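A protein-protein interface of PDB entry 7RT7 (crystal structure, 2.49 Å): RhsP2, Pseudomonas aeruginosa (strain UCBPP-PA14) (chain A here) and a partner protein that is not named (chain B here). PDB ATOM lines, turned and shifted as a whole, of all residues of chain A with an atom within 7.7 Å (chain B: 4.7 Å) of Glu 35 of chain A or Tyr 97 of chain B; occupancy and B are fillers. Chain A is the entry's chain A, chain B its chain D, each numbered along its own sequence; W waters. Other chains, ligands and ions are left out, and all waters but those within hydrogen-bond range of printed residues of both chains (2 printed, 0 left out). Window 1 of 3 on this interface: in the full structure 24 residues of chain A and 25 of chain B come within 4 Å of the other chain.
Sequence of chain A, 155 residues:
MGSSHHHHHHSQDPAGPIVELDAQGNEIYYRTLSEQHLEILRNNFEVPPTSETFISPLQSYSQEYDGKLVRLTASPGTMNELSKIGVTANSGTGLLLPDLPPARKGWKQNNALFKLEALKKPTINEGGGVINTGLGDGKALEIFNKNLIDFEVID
The backbone carbonyl oxygen (O) of Glu 35 of chain A lies within hydrogen-bond range of the side-chain hydroxyl (OH) of Tyr 97 of chain B, at 3.3 Å. NE2 of Gln 36 of chain A lies close to N of Thr 96 of chain B (3.3 Å). The guanidinium group of Arg 10 of chain B lies within salt-bridge range of the side-chain carboxylate of Glu 39 of chain A (2.6 Å). The side-chain carboxylate (OE1) of Glu 35 of chain A lies close to the side-chain carboxylate (OE1) of Glu 94 of chain B. The side-chain carboxylate (OE1) of Glu 35 of chain A lies close to the side-chain amino group (NZ) of Lys 135 of chain B (2.4 Å). N of Lys 135 of chain B sits close to NH1 of Arg 42 of chain A.
ND2 of Asn 43 of chain A lies within hydrogen-bond range of O of Glu 39 of chain A, 2.9 Å away. OH of Tyr 5 of chain B sits at hydrogen-bond distance from NH1 of Arg 10 of chain B, at 3.1 Å. The side-chain carboxylate of Glu 94 of chain B is in salt-bridge range of the side-chain amino group of Lys 135 of chain B, at 3.5 Å. The backbone carbonyl oxygen (O) of Tyr 97 of chain B sits at hydrogen-bond distance from the side-chain hydroxyl (OH) of Tyr 107 of chain B (3.0 Å).
Glu 35 of chain A touches Gly 95 of chain B (CG to N, 3.4 Å). Gln 36 of chain A touches Gly 95 of chain B (NE2 to C, 3.9 Å). OH of Tyr 97 of chain B touches CA of Gln 36 of chain A (3.3 Å). Glu 39 of chain A touches Tyr 97 of chain B (CB to OH, 3.5 Å).
Tyr 97 of chain B touches just these residues of chain A: Glu 35 (3.3 Å), Gln 36 (3.3 Å) and Glu 39 (3.5 Å). Of the printed residues of chain A, Glu 94 of chain B touches Glu 35. Of the printed residues of chain B, Gln 36 of chain A touches Gly 95, Thr 96 and Tyr 97. Thr 81 of chain B touches none of the printed residues of chain A. The nearest printed residue of chain A that does not touch Thr 96 of chain B is Glu 35 of chain A (6.0 Å).
Of the 15 printed residues of chain B, 6 touch a printed residue of chain A. Hydrophobic or aromatic side chains of chain B within 4 Å of the printed part of chain A: Tyr 97. Among the printed residues, 10 pairs touch across the chains. Among the printed residues, Asp or Glu carboxylates within 4 Å of a Lys or Arg side-chain nitrogen of the other chain: Glu 35 of chain A with Lys 135 of chain B (2.4 Å) and Glu 39 of chain A with Arg 10 of chain B (2.6 Å).
Water W1 lies within hydrogen-bond range of the backbone carbonyl oxygen of Gln 36 of chain A (2.4 Å), the side-chain carboxylate of Glu 39 of chain A (2.8 Å) and the guanidinium group of Arg 10 of chain B (3.1 Å). Water W2 lies within hydrogen-bond range of OH of Tyr 5 of chain B (2.5 Å), O of Val 137 of chain B (2.6 Å) and OE2 of Glu 39 of chain A (2.9 Å).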
ATOM      1  N   LEU A  33      31.960   8.023 -19.904  1.00  0.00           N
ATOM      2  CA  LEU A  33      30.824   7.623 -19.087  1.00  0.00           C
ATOM      3  C   LEU A  33      30.348   6.219 -19.429  1.00  0.00           C
ATOM      4  O   LEU A  33      30.647   5.669 -20.494  1.00  0.00           O
ATOM      5  CB  LEU A  33      29.645   8.597 -19.254  1.00  0.00           C
ATOM      6  CG  LEU A  33      29.654   9.806 -18.321  1.00  0.00           C
ATOM      7  CD1 LEU A  33      30.848  10.648 -18.649  1.00  0.00           C
ATOM      8  CD2 LEU A  33      28.406  10.662 -18.430  1.00  0.00           C
ATOM      9  N   SER A  34      29.583   5.655 -18.500  1.00  0.00           N
ATOM     10  CA  SER A  34      28.905   4.390 -18.707  1.00  0.00           C
ATOM     11  C   SER A  34      27.689   4.584 -19.610  1.00  0.00           C
ATOM     12  O   SER A  34      27.262   5.705 -19.899  1.00  0.00           O
ATOM     13  CB  SER A  34      28.477   3.794 -17.368  1.00  0.00           C
ATOM     14  OG  SER A  34      27.644   4.698 -16.660  1.00  0.00           O
ATOM     15  N   GLU A  35      27.125   3.461 -20.060  1.00  0.00           N
ATOM     16  CA  GLU A  35      25.909   3.521 -20.861  1.00  0.00           C
ATOM     17  C   GLU A  35      24.740   4.049 -20.039  1.00  0.00           C
ATOM     18  O   GLU A  35      23.951   4.870 -20.521  1.00  0.00           O
ATOM     19  CB  GLU A  35      25.583   2.138 -21.424  1.00  0.00           C
ATOM     20  CG  GLU A  35      26.699   1.518 -22.260  1.00  0.00           C
ATOM     21  CD  GLU A  35      26.483   1.684 -23.755  1.00  0.00           C
ATOM     22  OE1 GLU A  35      25.315   1.741 -24.192  1.00  0.00           O
ATOM     23  OE2 GLU A  35      27.487   1.754 -24.497  1.00  0.00           O
ATOM     24  N   GLN A  36      24.613   3.586 -18.792  1.00  0.00           N
ATOM     25  CA  GLN A  36      23.543   4.070 -17.927  1.00  0.00           C
ATOM     26  C   GLN A  36      23.652   5.573 -17.712  1.00  0.00           C
ATOM     27  O   GLN A  36      22.643   6.288 -17.734  1.00  0.00           O
ATOM     28  CB  GLN A  36      23.580   3.336 -16.588  1.00  0.00           C
ATOM     29  CG  GLN A  36      23.446   1.826 -16.703  1.00  0.00           C
ATOM     30  CD  GLN A  36      24.789   1.124 -16.744  1.00  0.00           C
ATOM     31  OE1 GLN A  36      25.780   1.682 -17.216  1.00  0.00           O
ATOM     32  NE2 GLN A  36      24.827  -0.108 -16.252  1.00  0.00           N
ATOM     33  N   HIS A  37      24.872   6.072 -17.498  1.00  0.00           N
ATOM     34  CA  HIS A  37      25.058   7.505 -17.300  1.00  0.00           C
ATOM     35  C   HIS A  37      24.842   8.279 -18.593  1.00  0.00           C
ATOM     36  O   HIS A  37      24.369   9.421 -18.560  1.00  0.00           O
ATOM     37  CB  HIS A  37      26.456   7.780 -16.745  1.00  0.00           C
ATOM     38  CG  HIS A  37      26.594   7.497 -15.281  1.00  0.00           C
ATOM     39  ND1 HIS A  37      25.523   7.173 -14.478  1.00  0.00           N
ATOM     40  CD2 HIS A  37      27.682   7.492 -14.474  1.00  0.00           C
ATOM     41  CE1 HIS A  37      25.943   6.977 -13.242  1.00  0.00           C
ATOM     42  NE2 HIS A  37      27.251   7.166 -13.212  1.00  0.00           N
ATOM     43  N   LEU A  38      25.180   7.679 -19.736  1.00  0.00           N
ATOM     44  CA  LEU A  38      24.977   8.352 -21.015  1.00  0.00           C
ATOM     45  C   LEU A  38      23.494   8.458 -21.349  1.00  0.00           C
ATOM     46  O   LEU A  38      23.054   9.453 -21.935  1.00  0.00           O
ATOM     47  CB  LEU A  38      25.731   7.611 -22.118  1.00  0.00           C
ATOM     48  CG  LEU A  38      25.824   8.270 -23.498  1.00  0.00           C
ATOM     49  CD1 LEU A  38      24.556   8.023 -24.308  1.00  0.00           C
ATOM     50  CD2 LEU A  38      26.108   9.762 -23.385  1.00  0.00           C
ATOM     51  N   GLU A  39      22.709   7.440 -20.987  1.00  0.00           N
ATOM     52  CA  GLU A  39      21.266   7.517 -21.186  1.00  0.00           C
ATOM     53  C   GLU A  39      20.679   8.713 -20.447  1.00  0.00           C
ATOM     54  O   GLU A  39      19.823   9.427 -20.981  1.00  0.00           O
ATOM     55  CB  GLU A  39      20.605   6.219 -20.720  1.00  0.00           C
ATOM     56  CG  GLU A  39      19.121   6.114 -21.041  1.00  0.00           C
ATOM     57  CD  GLU A  39      18.442   4.990 -20.282  1.00  0.00           C
ATOM     58  OE1 GLU A  39      18.360   5.075 -19.040  1.00  0.00           O
ATOM     59  OE2 GLU A  39      17.993   4.020 -20.927  1.00  0.00           O
ATOM     60  N   ILE A  40      21.136   8.947 -19.216  1.00  0.00           N
ATOM     61  CA  ILE A  40      20.653  10.085 -18.441  1.00  0.00           C
ATOM     62  C   ILE A  40      21.097  11.394 -19.081  1.00  0.00           C
ATOM     63  O   ILE A  40      20.354  12.383 -19.084  1.00  0.00           O
ATOM     64  CB  ILE A  40      21.145   9.974 -16.986  1.00  0.00           C
ATOM     65  CG1 ILE A  40      20.618   8.691 -16.337  1.00  0.00           C
ATOM     66  CG2 ILE A  40      20.719  11.191 -16.182  1.00  0.00           C
ATOM     67  CD1 ILE A  40      21.508   8.163 -15.234  1.00  0.00           C
ATOM     68  N   LEU A  41      22.312  11.424 -19.631  1.00  0.00           N
ATOM     69  CA  LEU A  41      22.830  12.659 -20.210  1.00  0.00           C
ATOM     70  C   LEU A  41      22.004  13.092 -21.413  1.00  0.00           C
ATOM     71  O   LEU A  41      21.763  14.288 -21.613  1.00  0.00           O
ATOM     72  CB  LEU A  41      24.296  12.475 -20.599  1.00  0.00           C
ATOM     73  CG  LEU A  41      25.017  13.689 -21.189  1.00  0.00           C
ATOM     74  CD1 LEU A  41      24.821  14.933 -20.332  1.00  0.00           C
ATOM     75  CD2 LEU A  41      26.497  13.376 -21.348  1.00  0.00           C
ATOM     76  N   ARG A  42      21.560  12.131 -22.228  1.00  0.00           N
ATOM     77  CA  ARG A  42      20.703  12.468 -23.358  1.00  0.00           C
ATOM     78  C   ARG A  42      19.319  12.900 -22.892  1.00  0.00           C
ATOM     79  O   ARG A  42      18.738  13.845 -23.438  1.00  0.00           O
ATOM     80  CB  ARG A  42      20.569  11.274 -24.301  1.00  0.00           C
ATOM     81  CG  ARG A  42      21.845  10.821 -24.981  1.00  0.00           C
ATOM     82  CD  ARG A  42      21.618   9.452 -25.596  1.00  0.00           C
ATOM     83  NE  ARG A  42      22.494   9.173 -26.727  1.00  0.00           N
ATOM     84  CZ  ARG A  42      22.751   7.956 -27.187  1.00  0.00           C
ATOM     85  NH1 ARG A  42      22.234   6.878 -26.621  1.00  0.00           N
ATOM     86  NH2 ARG A  42      23.546   7.817 -28.244  1.00  0.00           N
ATOM     87  N   ASN A  43      18.776  12.218 -21.883  1.00  0.00           N
ATOM     88  CA  ASN A  43      17.375  12.354 -21.516  1.00  0.00           C
ATOM     89  C   ASN A  43      17.133  13.304 -20.351  1.00  0.00           C
ATOM     90  O   ASN A  43      16.016  13.813 -20.214  1.00  0.00           O
ATOM     91  CB  ASN A  43      16.800  10.972 -21.176  1.00  0.00           C
ATOM     92  CG  ASN A  43      17.098   9.942 -22.253  1.00  0.00           C
ATOM     93  OD1 ASN A  43      17.285  10.288 -23.420  1.00  0.00           O
ATOM     94  ND2 ASN A  43      17.151   8.673 -21.867  1.00  0.00           N
ATOM     95  N   GLY A  67      34.510   3.377 -22.606  1.00  0.00           N
ATOM     96  CA  GLY A  67      33.154   3.865 -22.498  1.00  0.00           C
ATOM     97  C   GLY A  67      32.855   4.865 -23.591  1.00  0.00           C
ATOM     98  O   GLY A  67      33.535   4.912 -24.622  1.00  0.00           O
ATOM     99  N   LYS A  68      31.822   5.672 -23.360  1.00  0.00           N
ATOM    100  CA  LYS A  68      31.406   6.702 -24.307  1.00  0.00           C
ATOM    101  C   LYS A  68      32.119   8.003 -23.950  1.00  0.00           C
ATOM    102  O   LYS A  68      31.881   8.578 -22.883  1.00  0.00           O
ATOM    103  CB  LYS A  68      29.889   6.881 -24.278  1.00  0.00           C
ATOM    104  CG  LYS A  68      29.094   5.725 -24.886  1.00  0.00           C
ATOM    105  CD  LYS A  68      29.292   5.616 -26.395  1.00  0.00           C
ATOM    106  CE  LYS A  68      28.196   4.776 -27.047  1.00  0.00           C
ATOM    107  NZ  LYS A  68      27.339   5.565 -27.978  1.00  0.00           N
ATOM    108  N   ILE B   4      15.700  -9.462 -16.525  1.00  0.00           N
ATOM    109  CA  ILE B   4      16.602  -8.844 -15.558  1.00  0.00           C
ATOM    110  C   ILE B   4      16.466  -7.329 -15.542  1.00  0.00           C
ATOM    111  O   ILE B   4      16.974  -6.680 -14.613  1.00  0.00           O
ATOM    112  CB  ILE B   4      18.061  -9.247 -15.855  1.00  0.00           C
ATOM    113  CG1 ILE B   4      18.953  -8.976 -14.642  1.00  0.00           C
ATOM    114  CG2 ILE B   4      18.583  -8.506 -17.077  1.00  0.00           C
ATOM    115  CD1 ILE B   4      20.332  -9.597 -14.756  1.00  0.00           C
ATOM    116  N   TYR B   5      15.798  -6.745 -16.535  1.00  0.00           N
ATOM    117  CA  TYR B   5      15.560  -5.309 -16.570  1.00  0.00           C
ATOM    118  C   TYR B   5      14.362  -5.031 -17.465  1.00  0.00           C
ATOM    119  O   TYR B   5      14.249  -5.602 -18.554  1.00  0.00           O
ATOM    120  CB  TYR B   5      16.790  -4.552 -17.079  1.00  0.00           C
ATOM    121  CG  TYR B   5      16.522  -3.096 -17.384  1.00  0.00           C
ATOM    122  CD1 TYR B   5      16.523  -2.144 -16.372  1.00  0.00           C
ATOM    123  CD2 TYR B   5      16.265  -2.674 -18.681  1.00  0.00           C
ATOM    124  CE1 TYR B   5      16.282  -0.811 -16.646  1.00  0.00           C
ATOM    125  CE2 TYR B   5      16.020  -1.345 -18.962  1.00  0.00           C
ATOM    126  CZ  TYR B   5      16.030  -0.418 -17.943  1.00  0.00           C
ATOM    127  OH  TYR B   5      15.787   0.906 -18.224  1.00  0.00           O
ATOM    128  N   ARG B  10      11.441   0.585 -14.590  1.00  0.00           N
ATOM    129  CA  ARG B  10      12.256   1.790 -14.486  1.00  0.00           C
ATOM    130  C   ARG B  10      11.388   3.037 -14.394  1.00  0.00           C
ATOM    131  O   ARG B  10      11.754   4.000 -13.711  1.00  0.00           O
ATOM    132  CB  ARG B  10      13.198   1.878 -15.693  1.00  0.00           C
ATOM    133  CG  ARG B  10      13.819   3.251 -15.960  1.00  0.00           C
ATOM    134  CD  ARG B  10      14.902   3.601 -14.954  1.00  0.00           C
ATOM    135  NE  ARG B  10      15.766   4.671 -15.438  1.00  0.00           N
ATOM    136  CZ  ARG B  10      16.748   4.507 -16.314  1.00  0.00           C
ATOM    137  NH1 ARG B  10      17.031   3.317 -16.821  1.00  0.00           N
ATOM    138  NH2 ARG B  10      17.466   5.562 -16.690  1.00  0.00           N
ATOM    139  N   THR B  81      28.954  -2.848 -17.786  1.00  0.00           N
ATOM    140  CA  THR B  81      28.812  -2.949 -19.234  1.00  0.00           C
ATOM    141  C   THR B  81      29.066  -4.382 -19.672  1.00  0.00           C
ATOM    142  O   THR B  81      29.832  -5.113 -19.040  1.00  0.00           O
ATOM    143  CB  THR B  81      29.781  -2.003 -19.959  1.00  0.00           C
ATOM    144  OG1 THR B  81      29.492  -0.653 -19.584  1.00  0.00           O
ATOM    145  CG2 THR B  81      29.667  -2.142 -21.471  1.00  0.00           C
ATOM    146  N   THR B  93      27.500  -3.659 -27.540  1.00  0.00           N
ATOM    147  CA  THR B  93      27.905  -3.250 -26.203  1.00  0.00           C
ATOM    148  C   THR B  93      26.734  -2.538 -25.543  1.00  0.00           C
ATOM    149  O   THR B  93      26.113  -1.663 -26.156  1.00  0.00           O
ATOM    150  CB  THR B  93      29.127  -2.325 -26.251  1.00  0.00           C
ATOM    151  OG1 THR B  93      30.191  -2.966 -26.969  1.00  0.00           O
ATOM    152  CG2 THR B  93      29.602  -1.983 -24.844  1.00  0.00           C
ATOM    153  N   GLU B  94      26.432  -2.910 -24.301  1.00  0.00           N
ATOM    154  CA  GLU B  94      25.307  -2.315 -23.597  1.00  0.00           C
ATOM    155  C   GLU B  94      25.586  -2.300 -22.103  1.00  0.00           C
ATOM    156  O   GLU B  94      26.317  -3.144 -21.580  1.00  0.00           O
ATOM    157  CB  GLU B  94      24.002  -3.074 -23.871  1.00  0.00           C
ATOM    158  CG  GLU B  94      22.776  -2.413 -23.265  1.00  0.00           C
ATOM    159  CD  GLU B  94      22.626  -0.968 -23.696  1.00  0.00           C
ATOM    160  OE1 GLU B  94      23.024  -0.646 -24.835  1.00  0.00           O
ATOM    161  OE2 GLU B  94      22.123  -0.154 -22.897  1.00  0.00           O
ATOM    162  N   GLY B  95      24.989  -1.323 -21.424  1.00  0.00           N
ATOM    163  CA  GLY B  95      25.086  -1.270 -19.982  1.00  0.00           C
ATOM    164  C   GLY B  95      24.334  -2.413 -19.326  1.00  0.00           C
ATOM    165  O   GLY B  95      23.365  -2.947 -19.865  1.00  0.00           O
ATOM    166  N   THR B  96      24.798  -2.791 -18.136  1.00  0.00           N
ATOM    167  CA  THR B  96      24.200  -3.896 -17.390  1.00  0.00           C
ATOM    168  C   THR B  96      23.046  -3.366 -16.538  1.00  0.00           C
ATOM    169  O   THR B  96      23.109  -3.289 -15.310  1.00  0.00           O
ATOM    170  CB  THR B  96      25.251  -4.592 -16.534  1.00  0.00           C
ATOM    171  OG1 THR B  96      25.764  -3.674 -15.560  1.00  0.00           O
ATOM    172  CG2 THR B  96      26.391  -5.094 -17.403  1.00  0.00           C
ATOM    173  N   TYR B  97      21.972  -2.994 -17.226  1.00  0.00           N
ATOM    174  CA  TYR B  97      20.810  -2.457 -16.534  1.00  0.00           C
ATOM    175  C   TYR B  97      20.157  -3.534 -15.676  1.00  0.00           C
ATOM    176  O   TYR B  97      20.026  -4.691 -16.087  1.00  0.00           O
ATOM    177  CB  TYR B  97      19.791  -1.906 -17.528  1.00  0.00           C
ATOM    178  CG  TYR B  97      20.223  -0.637 -18.226  1.00  0.00           C
ATOM    179  CD1 TYR B  97      21.089  -0.682 -19.308  1.00  0.00           C
ATOM    180  CD2 TYR B  97      19.758   0.602 -17.808  1.00  0.00           C
ATOM    181  CE1 TYR B  97      21.485   0.473 -19.952  1.00  0.00           C
ATOM    182  CE2 TYR B  97      20.146   1.763 -18.447  1.00  0.00           C
ATOM    183  CZ  TYR B  97      21.011   1.693 -19.518  1.00  0.00           C
ATOM    184  OH  TYR B  97      21.403   2.845 -20.160  1.00  0.00           O
ATOM    185  N   THR B  98      19.753  -3.140 -14.472  1.00  0.00           N
ATOM    186  CA  THR B  98      19.005  -3.996 -13.566  1.00  0.00           C
ATOM    187  C   THR B  98      17.965  -3.136 -12.865  1.00  0.00           C
ATOM    188  O   THR B  98      18.078  -1.909 -12.818  1.00  0.00           O
ATOM    189  CB  THR B  98      19.909  -4.673 -12.524  1.00  0.00           C
ATOM    190  OG1 THR B  98      20.795  -3.703 -11.950  1.00  0.00           O
ATOM    191  CG2 THR B  98      20.724  -5.791 -13.155  1.00  0.00           C
ATOM    192  N   ASN B  99      16.940  -3.784 -12.330  1.00  0.00           N
ATOM    193  CA  ASN B  99      15.971  -3.078 -11.511  1.00  0.00           C
ATOM    194  C   ASN B  99      16.410  -3.113 -10.050  1.00  0.00           C
ATOM    195  O   ASN B  99      17.341  -3.825  -9.668  1.00  0.00           O
ATOM    196  CB  ASN B  99      14.580  -3.687 -11.670  1.00  0.00           C
ATOM    197  CG  ASN B  99      14.078  -3.627 -13.098  1.00  0.00           C
ATOM    198  OD1 ASN B  99      13.911  -4.655 -13.755  1.00  0.00           O
ATOM    199  ND2 ASN B  99      13.831  -2.418 -13.588  1.00  0.00           N
ATOM    200  N   TYR B 107      24.528 -11.377 -14.345  1.00  0.00           N
ATOM    201  CA  TYR B 107      25.293 -11.153 -15.566  1.00  0.00           C
ATOM    202  C   TYR B 107      26.609 -11.919 -15.483  1.00  0.00           C
ATOM    203  O   TYR B 107      27.496 -11.559 -14.702  1.00  0.00           O
ATOM    204  CB  TYR B 107      25.554  -9.663 -15.766  1.00  0.00           C
ATOM    205  CG  TYR B 107      24.390  -8.883 -16.336  1.00  0.00           C
ATOM    206  CD1 TYR B 107      24.024  -9.012 -17.670  1.00  0.00           C
ATOM    207  CD2 TYR B 107      23.669  -8.002 -15.542  1.00  0.00           C
ATOM    208  CE1 TYR B 107      22.964  -8.294 -18.194  1.00  0.00           C
ATOM    209  CE2 TYR B 107      22.608  -7.278 -16.057  1.00  0.00           C
ATOM    210  CZ  TYR B 107      22.261  -7.427 -17.382  1.00  0.00           C
ATOM    211  OH  TYR B 107      21.206  -6.707 -17.893  1.00  0.00           O
ATOM    212  N   LYS B 135      19.292   5.950 -27.639  1.00  0.00           N
ATOM    213  CA  LYS B 135      19.074   4.513 -27.533  1.00  0.00           C
ATOM    214  C   LYS B 135      18.452   4.190 -26.182  1.00  0.00           C
ATOM    215  O   LYS B 135      19.080   4.394 -25.137  1.00  0.00           O
ATOM    216  CB  LYS B 135      20.395   3.770 -27.711  1.00  0.00           C
ATOM    217  CG  LYS B 135      20.307   2.259 -27.529  1.00  0.00           C
ATOM    218  CD  LYS B 135      21.691   1.638 -27.372  1.00  0.00           C
ATOM    219  CE  LYS B 135      22.366   2.099 -26.087  1.00  0.00           C
ATOM    220  NZ  LYS B 135      23.575   1.297 -25.762  1.00  0.00           N
ATOM    221  N   VAL B 137      16.913   1.332 -23.805  1.00  0.00           N
ATOM    222  CA  VAL B 137      16.732  -0.077 -23.479  1.00  0.00           C
ATOM    223  C   VAL B 137      15.334  -0.262 -22.906  1.00  0.00           C
ATOM    224  O   VAL B 137      14.969   0.370 -21.907  1.00  0.00           O
ATOM    225  CB  VAL B 137      17.804  -0.549 -22.487  1.00  0.00           C
ATOM    226  CG1 VAL B 137      17.547  -1.987 -22.061  1.00  0.00           C
ATOM    227  CG2 VAL B 137      19.188  -0.407 -23.093  1.00  0.00           C
ATOM    228  N   ILE B 140      15.650  -6.326 -20.928  1.00  0.00           N
ATOM    229  CA  ILE B 140      16.815  -7.200 -20.978  1.00  0.00           C
ATOM    230  C   ILE B 140      16.414  -8.537 -20.369  1.00  0.00           C
ATOM    231  O   ILE B 140      15.942  -8.584 -19.227  1.00  0.00           O
ATOM    232  CB  ILE B 140      18.021  -6.611 -20.226  1.00  0.00           C
ATOM    233  CG1 ILE B 140      18.404  -5.249 -20.812  1.00  0.00           C
ATOM    234  CG2 ILE B 140      19.199  -7.576 -20.283  1.00  0.00           C
ATOM    235  CD1 ILE B 140      19.563  -4.577 -20.099  1.00  0.00           C
HETATM  236  O   HOH W   1      20.545   5.176 -17.219  1.00  0.00           O
HETATM  237  O   HOH W   2      15.838   2.211 -20.336  1.00  0.00           O
